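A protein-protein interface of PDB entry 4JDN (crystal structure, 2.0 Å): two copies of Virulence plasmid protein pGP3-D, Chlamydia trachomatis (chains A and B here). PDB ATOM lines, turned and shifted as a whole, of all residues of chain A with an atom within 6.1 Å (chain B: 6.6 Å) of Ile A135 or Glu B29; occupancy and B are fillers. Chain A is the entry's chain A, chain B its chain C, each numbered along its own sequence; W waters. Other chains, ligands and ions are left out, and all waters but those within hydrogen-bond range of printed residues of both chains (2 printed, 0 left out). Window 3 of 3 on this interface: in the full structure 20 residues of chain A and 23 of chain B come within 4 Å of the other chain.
The side-chain hydroxyl (OH) of Tyr B83 is in hydrogen-bond range of the side-chain amide oxygen (OD1) of Asn A137 (2.7 Å).
N of Ser B26 sits close to OG1 of Thr B24 (3.3 Å).
O of Ile A135 is in hydrogen-bond range of ND2 of Asn A137 (3.1 Å).
The backbone carbonyl oxygen (O) of Ile A132 sits at hydrogen-bond distance from the side-chain amide nitrogen (ND2) of Asn A137 (3.1 Å).
The backbone NH of Thr B24 sits at hydrogen-bond distance from the side-chain amide oxygen of Asn B27.
Among the printed residues, pairs that only touch across the chains: Ile A132 with Tyr B83, Ile A135 with Ile B81, Leu A133 with Ile B28, Ile A135 with Glu B29, Leu A133 with Thr B24, Leu A133 with Pro B25, Leu A133 with Tyr B83 and Ile A135 with Ile B28.
Glu B29 touches just one residue of chain A: Ile A135.
Of the printed residues of chain A, Ile B81 touches Ile A135.
Of the printed residues of chain B, Asn A137 touches Tyr B83.
Printed residues of chain A within 4 Å of Pro B25: Leu A133.
Gly A134 touches none of the printed residues of chain B.
The nearest residue of chain A that does not touch Glu B29 is Gly A134 (5.7 Å).
Hydrophobic or aromatic side chains of chain A within 4 Å of the printed part of chain B: Ile A132, Leu A133 and Ile A135.
Printed residues of chain B that touch a printed residue of chain A: Thr B24, Pro B25, Ile B28, Glu B29, Ile B81 and Tyr B83.
Among the printed residues, 9 pairs touch across the chains.
No position is printed for both chains.
Of the 9 pairs that touch across the chains among the printed residues, none has its exchanged pair printed and touching as well.
Water W2 bridges the backbone carbonyl oxygen (O) of Pro B25 (2.7 Å) and the backbone carbonyl oxygen (O) of Leu A133 (2.8 Å).
Water W1 lies within hydrogen-bond range of the backbone carbonyl oxygen (O) of Ile B81 and the side-chain amide oxygen (OD1) of Asn A137.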
ATOM      1  N   ASN A 124      28.512 -21.375  33.541  1.00  0.00           N
ATOM      2  CA  ASN A 124      27.655 -21.583  32.359  1.00  0.00           C
ATOM      3  C   ASN A 124      28.148 -20.896  31.071  1.00  0.00           C
ATOM      4  O   ASN A 124      27.350 -20.547  30.199  1.00  0.00           O
ATOM      5  CB  ASN A 124      26.210 -21.152  32.630  1.00  0.00           C
ATOM      6  CG  ASN A 124      25.513 -22.017  33.669  1.00  0.00           C
ATOM      7  OD1 ASN A 124      25.723 -23.233  33.729  1.00  0.00           O
ATOM      8  ND2 ASN A 124      24.648 -21.393  34.476  1.00  0.00           N
ATOM      9  N   ASP A 131      28.852 -18.175  25.056  1.00  0.00           N
ATOM     10  CA  ASP A 131      27.996 -19.356  25.197  1.00  0.00           C
ATOM     11  C   ASP A 131      28.775 -20.618  24.860  1.00  0.00           C
ATOM     12  O   ASP A 131      29.511 -20.642  23.884  1.00  0.00           O
ATOM     13  CB  ASP A 131      26.820 -19.286  24.224  1.00  0.00           C
ATOM     14  CG  ASP A 131      25.885 -18.128  24.507  1.00  0.00           C
ATOM     15  OD1 ASP A 131      25.767 -17.726  25.680  1.00  0.00           O
ATOM     16  OD2 ASP A 131      25.243 -17.644  23.554  1.00  0.00           O
ATOM     17  N   ILE A 132      28.600 -21.675  25.647  1.00  0.00           N
ATOM     18  CA  ILE A 132      29.253 -22.931  25.315  1.00  0.00           C
ATOM     19  C   ILE A 132      28.449 -23.577  24.202  1.00  0.00           C
ATOM     20  O   ILE A 132      27.229 -23.712  24.325  1.00  0.00           O
ATOM     21  CB  ILE A 132      29.327 -23.882  26.540  1.00  0.00           C
ATOM     22  CG1 ILE A 132      30.029 -23.171  27.707  1.00  0.00           C
ATOM     23  CG2 ILE A 132      30.064 -25.163  26.164  1.00  0.00           C
ATOM     24  CD1 ILE A 132      29.653 -23.718  29.082  1.00  0.00           C
ATOM     25  N   LEU A 133      29.128 -23.953  23.115  1.00  0.00           N
ATOM     26  CA  LEU A 133      28.489 -24.549  21.934  1.00  0.00           C
ATOM     27  C   LEU A 133      27.350 -23.670  21.379  1.00  0.00           C
ATOM     28  O   LEU A 133      26.413 -24.155  20.738  1.00  0.00           O
ATOM     29  CB  LEU A 133      28.009 -25.979  22.222  1.00  0.00           C
ATOM     30  CG  LEU A 133      29.098 -27.046  22.423  1.00  0.00           C
ATOM     31  CD1 LEU A 133      28.493 -28.380  22.883  1.00  0.00           C
ATOM     32  CD2 LEU A 133      29.915 -27.231  21.136  1.00  0.00           C
ATOM     33  N   GLY A 134      27.444 -22.377  21.652  1.00  0.00           N
ATOM     34  CA  GLY A 134      26.499 -21.400  21.145  1.00  0.00           C
ATOM     35  C   GLY A 134      25.111 -21.481  21.735  1.00  0.00           C
ATOM     36  O   GLY A 134      24.184 -20.888  21.199  1.00  0.00           O
ATOM     37  N   ILE A 135      24.946 -22.203  22.838  1.00  0.00           N
ATOM     38  CA  ILE A 135      23.621 -22.338  23.436  1.00  0.00           C
ATOM     39  C   ILE A 135      23.593 -21.922  24.907  1.00  0.00           C
ATOM     40  O   ILE A 135      24.640 -21.748  25.535  1.00  0.00           O
ATOM     41  CB  ILE A 135      23.092 -23.788  23.338  1.00  0.00           C
ATOM     42  CG1 ILE A 135      24.019 -24.745  24.101  1.00  0.00           C
ATOM     43  CG2 ILE A 135      22.963 -24.210  21.880  1.00  0.00           C
ATOM     44  CD1 ILE A 135      23.389 -26.089  24.408  1.00  0.00           C
ATOM     45  N   THR A 136      22.384 -21.773  25.436  1.00  0.00           N
ATOM     46  CA  THR A 136      22.172 -21.635  26.877  1.00  0.00           C
ATOM     47  C   THR A 136      22.400 -22.986  27.549  1.00  0.00           C
ATOM     48  O   THR A 136      21.930 -24.025  27.078  1.00  0.00           O
ATOM     49  CB  THR A 136      20.761 -21.128  27.202  1.00  0.00           C
ATOM     50  OG1 THR A 136      20.635 -19.794  26.702  1.00  0.00           O
ATOM     51  CG2 THR A 136      20.513 -21.124  28.734  1.00  0.00           C
ATOM     52  N   ASN A 137      23.151 -22.954  28.636  1.00  0.00           N
ATOM     53  CA  ASN A 137      23.503 -24.144  29.384  1.00  0.00           C
ATOM     54  C   ASN A 137      22.963 -24.084  30.812  1.00  0.00           C
ATOM     55  O   ASN A 137      22.649 -23.013  31.319  1.00  0.00           O
ATOM     56  CB  ASN A 137      25.019 -24.320  29.354  1.00  0.00           C
ATOM     57  CG  ASN A 137      25.488 -24.891  28.037  1.00  0.00           C
ATOM     58  OD1 ASN A 137      25.339 -26.085  27.796  1.00  0.00           O
ATOM     59  ND2 ASN A 137      26.013 -24.040  27.163  1.00  0.00           N
ATOM     60  N   THR B  24      29.204 -30.229  18.336  1.00  0.00           N
ATOM     61  CA  THR B  24      29.610 -28.972  17.712  1.00  0.00           C
ATOM     62  C   THR B  24      28.475 -27.959  17.808  1.00  0.00           C
ATOM     63  O   THR B  24      27.340 -28.335  18.093  1.00  0.00           O
ATOM     64  CB  THR B  24      29.952 -29.173  16.216  1.00  0.00           C
ATOM     65  OG1 THR B  24      28.759 -29.515  15.500  1.00  0.00           O
ATOM     66  CG2 THR B  24      31.011 -30.257  16.035  1.00  0.00           C
ATOM     67  N   PRO B  25      28.767 -26.670  17.551  1.00  0.00           N
ATOM     68  CA  PRO B  25      27.655 -25.709  17.612  1.00  0.00           C
ATOM     69  C   PRO B  25      26.571 -26.033  16.589  1.00  0.00           C
ATOM     70  O   PRO B  25      25.412 -25.685  16.803  1.00  0.00           O
ATOM     71  CB  PRO B  25      28.327 -24.368  17.292  1.00  0.00           C
ATOM     72  CG  PRO B  25      29.748 -24.548  17.755  1.00  0.00           C
ATOM     73  CD  PRO B  25      30.072 -25.994  17.416  1.00  0.00           C
ATOM     74  N   SER B  26      26.943 -26.733  15.518  1.00  0.00           N
ATOM     75  CA  SER B  26      25.997 -27.126  14.480  1.00  0.00           C
ATOM     76  C   SER B  26      25.081 -28.275  14.881  1.00  0.00           C
ATOM     77  O   SER B  26      23.898 -28.265  14.544  1.00  0.00           O
ATOM     78  CB  SER B  26      26.738 -27.474  13.182  1.00  0.00           C
ATOM     79  OG  SER B  26      27.375 -26.318  12.664  1.00  0.00           O
ATOM     80  N   ASN B  27      25.604 -29.265  15.600  1.00  0.00           N
ATOM     81  CA  ASN B  27      24.790 -30.442  15.936  1.00  0.00           C
ATOM     82  C   ASN B  27      24.249 -30.541  17.378  1.00  0.00           C
ATOM     83  O   ASN B  27      23.472 -31.448  17.686  1.00  0.00           O
ATOM     84  CB  ASN B  27      25.520 -31.743  15.534  1.00  0.00           C
ATOM     85  CG  ASN B  27      26.703 -32.082  16.452  1.00  0.00           C
ATOM     86  OD1 ASN B  27      26.822 -31.559  17.568  1.00  0.00           O
ATOM     87  ND2 ASN B  27      27.578 -32.981  15.985  1.00  0.00           N
ATOM     88  N   ILE B  28      24.674 -29.632  18.257  1.00  0.00           N
ATOM     89  CA  ILE B  28      24.335 -29.724  19.680  1.00  0.00           C
ATOM     90  C   ILE B  28      22.823 -29.730  19.934  1.00  0.00           C
ATOM     91  O   ILE B  28      22.334 -30.498  20.759  1.00  0.00           O
ATOM     92  CB  ILE B  28      25.068 -28.638  20.544  1.00  0.00           C
ATOM     93  CG1 ILE B  28      24.776 -28.834  22.042  1.00  0.00           C
ATOM     94  CG2 ILE B  28      24.716 -27.226  20.086  1.00  0.00           C
ATOM     95  CD1 ILE B  28      25.162 -30.215  22.564  1.00  0.00           C
ATOM     96  N   GLU B  29      22.075 -28.908  19.201  1.00  0.00           N
ATOM     97  CA  GLU B  29      20.615 -28.950  19.294  1.00  0.00           C
ATOM     98  C   GLU B  29      19.972 -29.795  18.181  1.00  0.00           C
ATOM     99  O   GLU B  29      18.968 -29.400  17.575  1.00  0.00           O
ATOM    100  CB  GLU B  29      20.024 -27.534  19.333  1.00  0.00           C
ATOM    101  CG  GLU B  29      20.420 -26.754  20.578  1.00  0.00           C
ATOM    102  CD  GLU B  29      19.744 -25.394  20.676  1.00  0.00           C
ATOM    103  OE1 GLU B  29      19.994 -24.536  19.805  1.00  0.00           O
ATOM    104  OE2 GLU B  29      18.966 -25.185  21.626  1.00  0.00           O
ATOM    105  N   THR B  30      20.565 -30.954  17.909  1.00  0.00           N
ATOM    106  CA  THR B  30      19.981 -31.927  16.990  1.00  0.00           C
ATOM    107  C   THR B  30      20.012 -33.304  17.643  1.00  0.00           C
ATOM    108  O   THR B  30      20.219 -33.419  18.848  1.00  0.00           O
ATOM    109  CB  THR B  30      20.728 -31.987  15.630  1.00  0.00           C
ATOM    110  OG1 THR B  30      21.980 -32.667  15.785  1.00  0.00           O
ATOM    111  CG2 THR B  30      20.981 -30.595  15.086  1.00  0.00           C
ATOM    112  N   LEU B  31      19.813 -34.352  16.854  1.00  0.00           N
ATOM    113  CA  LEU B  31      19.910 -35.709  17.382  1.00  0.00           C
ATOM    114  C   LEU B  31      21.197 -36.377  16.930  1.00  0.00           C
ATOM    115  O   LEU B  31      21.401 -37.557  17.196  1.00  0.00           O
ATOM    116  CB  LEU B  31      18.715 -36.556  16.944  1.00  0.00           C
ATOM    117  CG  LEU B  31      17.353 -36.137  17.494  1.00  0.00           C
ATOM    118  CD1 LEU B  31      16.253 -36.975  16.876  1.00  0.00           C
ATOM    119  CD2 LEU B  31      17.348 -36.290  18.995  1.00  0.00           C
ATOM    120  N   LEU B  32      22.067 -35.615  16.270  1.00  0.00           N
ATOM    121  CA  LEU B  32      23.241 -36.175  15.606  1.00  0.00           C
ATOM    122  C   LEU B  32      24.543 -36.055  16.405  1.00  0.00           C
ATOM    123  O   LEU B  32      25.561 -36.616  16.010  1.00  0.00           O
ATOM    124  CB  LEU B  32      23.443 -35.488  14.259  1.00  0.00           C
ATOM    125  CG  LEU B  32      22.216 -35.330  13.361  1.00  0.00           C
ATOM    126  CD1 LEU B  32      22.615 -34.563  12.119  1.00  0.00           C
ATOM    127  CD2 LEU B  32      21.621 -36.681  12.999  1.00  0.00           C
ATOM    128  N   SER B  76      13.461 -33.653  19.446  1.00  0.00           N
ATOM    129  CA  SER B  76      14.342 -33.392  18.316  1.00  0.00           C
ATOM    130  C   SER B  76      15.707 -32.848  18.751  1.00  0.00           C
ATOM    131  O   SER B  76      16.557 -32.549  17.912  1.00  0.00           O
ATOM    132  CB  SER B  76      13.680 -32.406  17.349  1.00  0.00           C
ATOM    133  OG  SER B  76      13.645 -31.114  17.926  1.00  0.00           O
ATOM    134  N   LYS B  77      15.910 -32.721  20.059  1.00  0.00           N
ATOM    135  CA  LYS B  77      17.182 -32.236  20.604  1.00  0.00           C
ATOM    136  C   LYS B  77      17.301 -32.657  22.076  1.00  0.00           C
ATOM    137  O   LYS B  77      16.325 -33.124  22.664  1.00  0.00           O
ATOM    138  CB  LYS B  77      17.298 -30.716  20.424  1.00  0.00           C
ATOM    139  CG  LYS B  77      16.280 -29.900  21.184  1.00  0.00           C
ATOM    140  CD  LYS B  77      16.464 -28.418  20.894  1.00  0.00           C
ATOM    141  CE  LYS B  77      15.663 -27.578  21.872  1.00  0.00           C
ATOM    142  NZ  LYS B  77      14.233 -27.999  21.875  1.00  0.00           N
ATOM    143  N   PRO B  78      18.503 -32.532  22.667  1.00  0.00           N
ATOM    144  CA  PRO B  78      18.671 -33.008  24.052  1.00  0.00           C
ATOM    145  C   PRO B  78      17.829 -32.216  25.050  1.00  0.00           C
ATOM    146  O   PRO B  78      17.548 -31.056  24.791  1.00  0.00           O
ATOM    147  CB  PRO B  78      20.166 -32.766  24.327  1.00  0.00           C
ATOM    148  CG  PRO B  78      20.817 -32.745  22.961  1.00  0.00           C
ATOM    149  CD  PRO B  78      19.786 -32.123  22.056  1.00  0.00           C
ATOM    150  N   ILE B  81      22.220 -31.197  28.937  1.00  0.00           N
ATOM    151  CA  ILE B  81      23.561 -31.241  28.404  1.00  0.00           C
ATOM    152  C   ILE B  81      24.545 -30.930  29.537  1.00  0.00           C
ATOM    153  O   ILE B  81      24.342 -29.996  30.313  1.00  0.00           O
ATOM    154  CB  ILE B  81      23.729 -30.218  27.265  1.00  0.00           C
ATOM    155  CG1 ILE B  81      22.847 -30.616  26.073  1.00  0.00           C
ATOM    156  CG2 ILE B  81      25.188 -30.118  26.840  1.00  0.00           C
ATOM    157  CD1 ILE B  81      22.610 -29.494  25.073  1.00  0.00           C
ATOM    158  N   TYR B  83      29.027 -31.330  30.891  1.00  0.00           N
ATOM    159  CA  TYR B  83      30.408 -31.240  30.410  1.00  0.00           C
ATOM    160  C   TYR B  83      31.367 -31.906  31.377  1.00  0.00           C
ATOM    161  O   TYR B  83      31.209 -31.801  32.595  1.00  0.00           O
ATOM    162  CB  TYR B  83      30.805 -29.770  30.217  1.00  0.00           C
ATOM    163  CG  TYR B  83      29.907 -29.088  29.213  1.00  0.00           C
ATOM    164  CD1 TYR B  83      30.173 -29.174  27.845  1.00  0.00           C
ATOM    165  CD2 TYR B  83      28.762 -28.417  29.626  1.00  0.00           C
ATOM    166  CE1 TYR B  83      29.322 -28.594  26.910  1.00  0.00           C
ATOM    167  CE2 TYR B  83      27.904 -27.836  28.710  1.00  0.00           C
ATOM    168  CZ  TYR B  83      28.197 -27.919  27.346  1.00  0.00           C
ATOM    169  OH  TYR B  83      27.349 -27.332  26.429  1.00  0.00           O
HETATM  170  O   HOH W   1      23.719 -27.421  29.613  1.00  0.00           O
HETATM  171  O   HOH W   2      24.613 -23.891  18.666  1.00  0.00           O
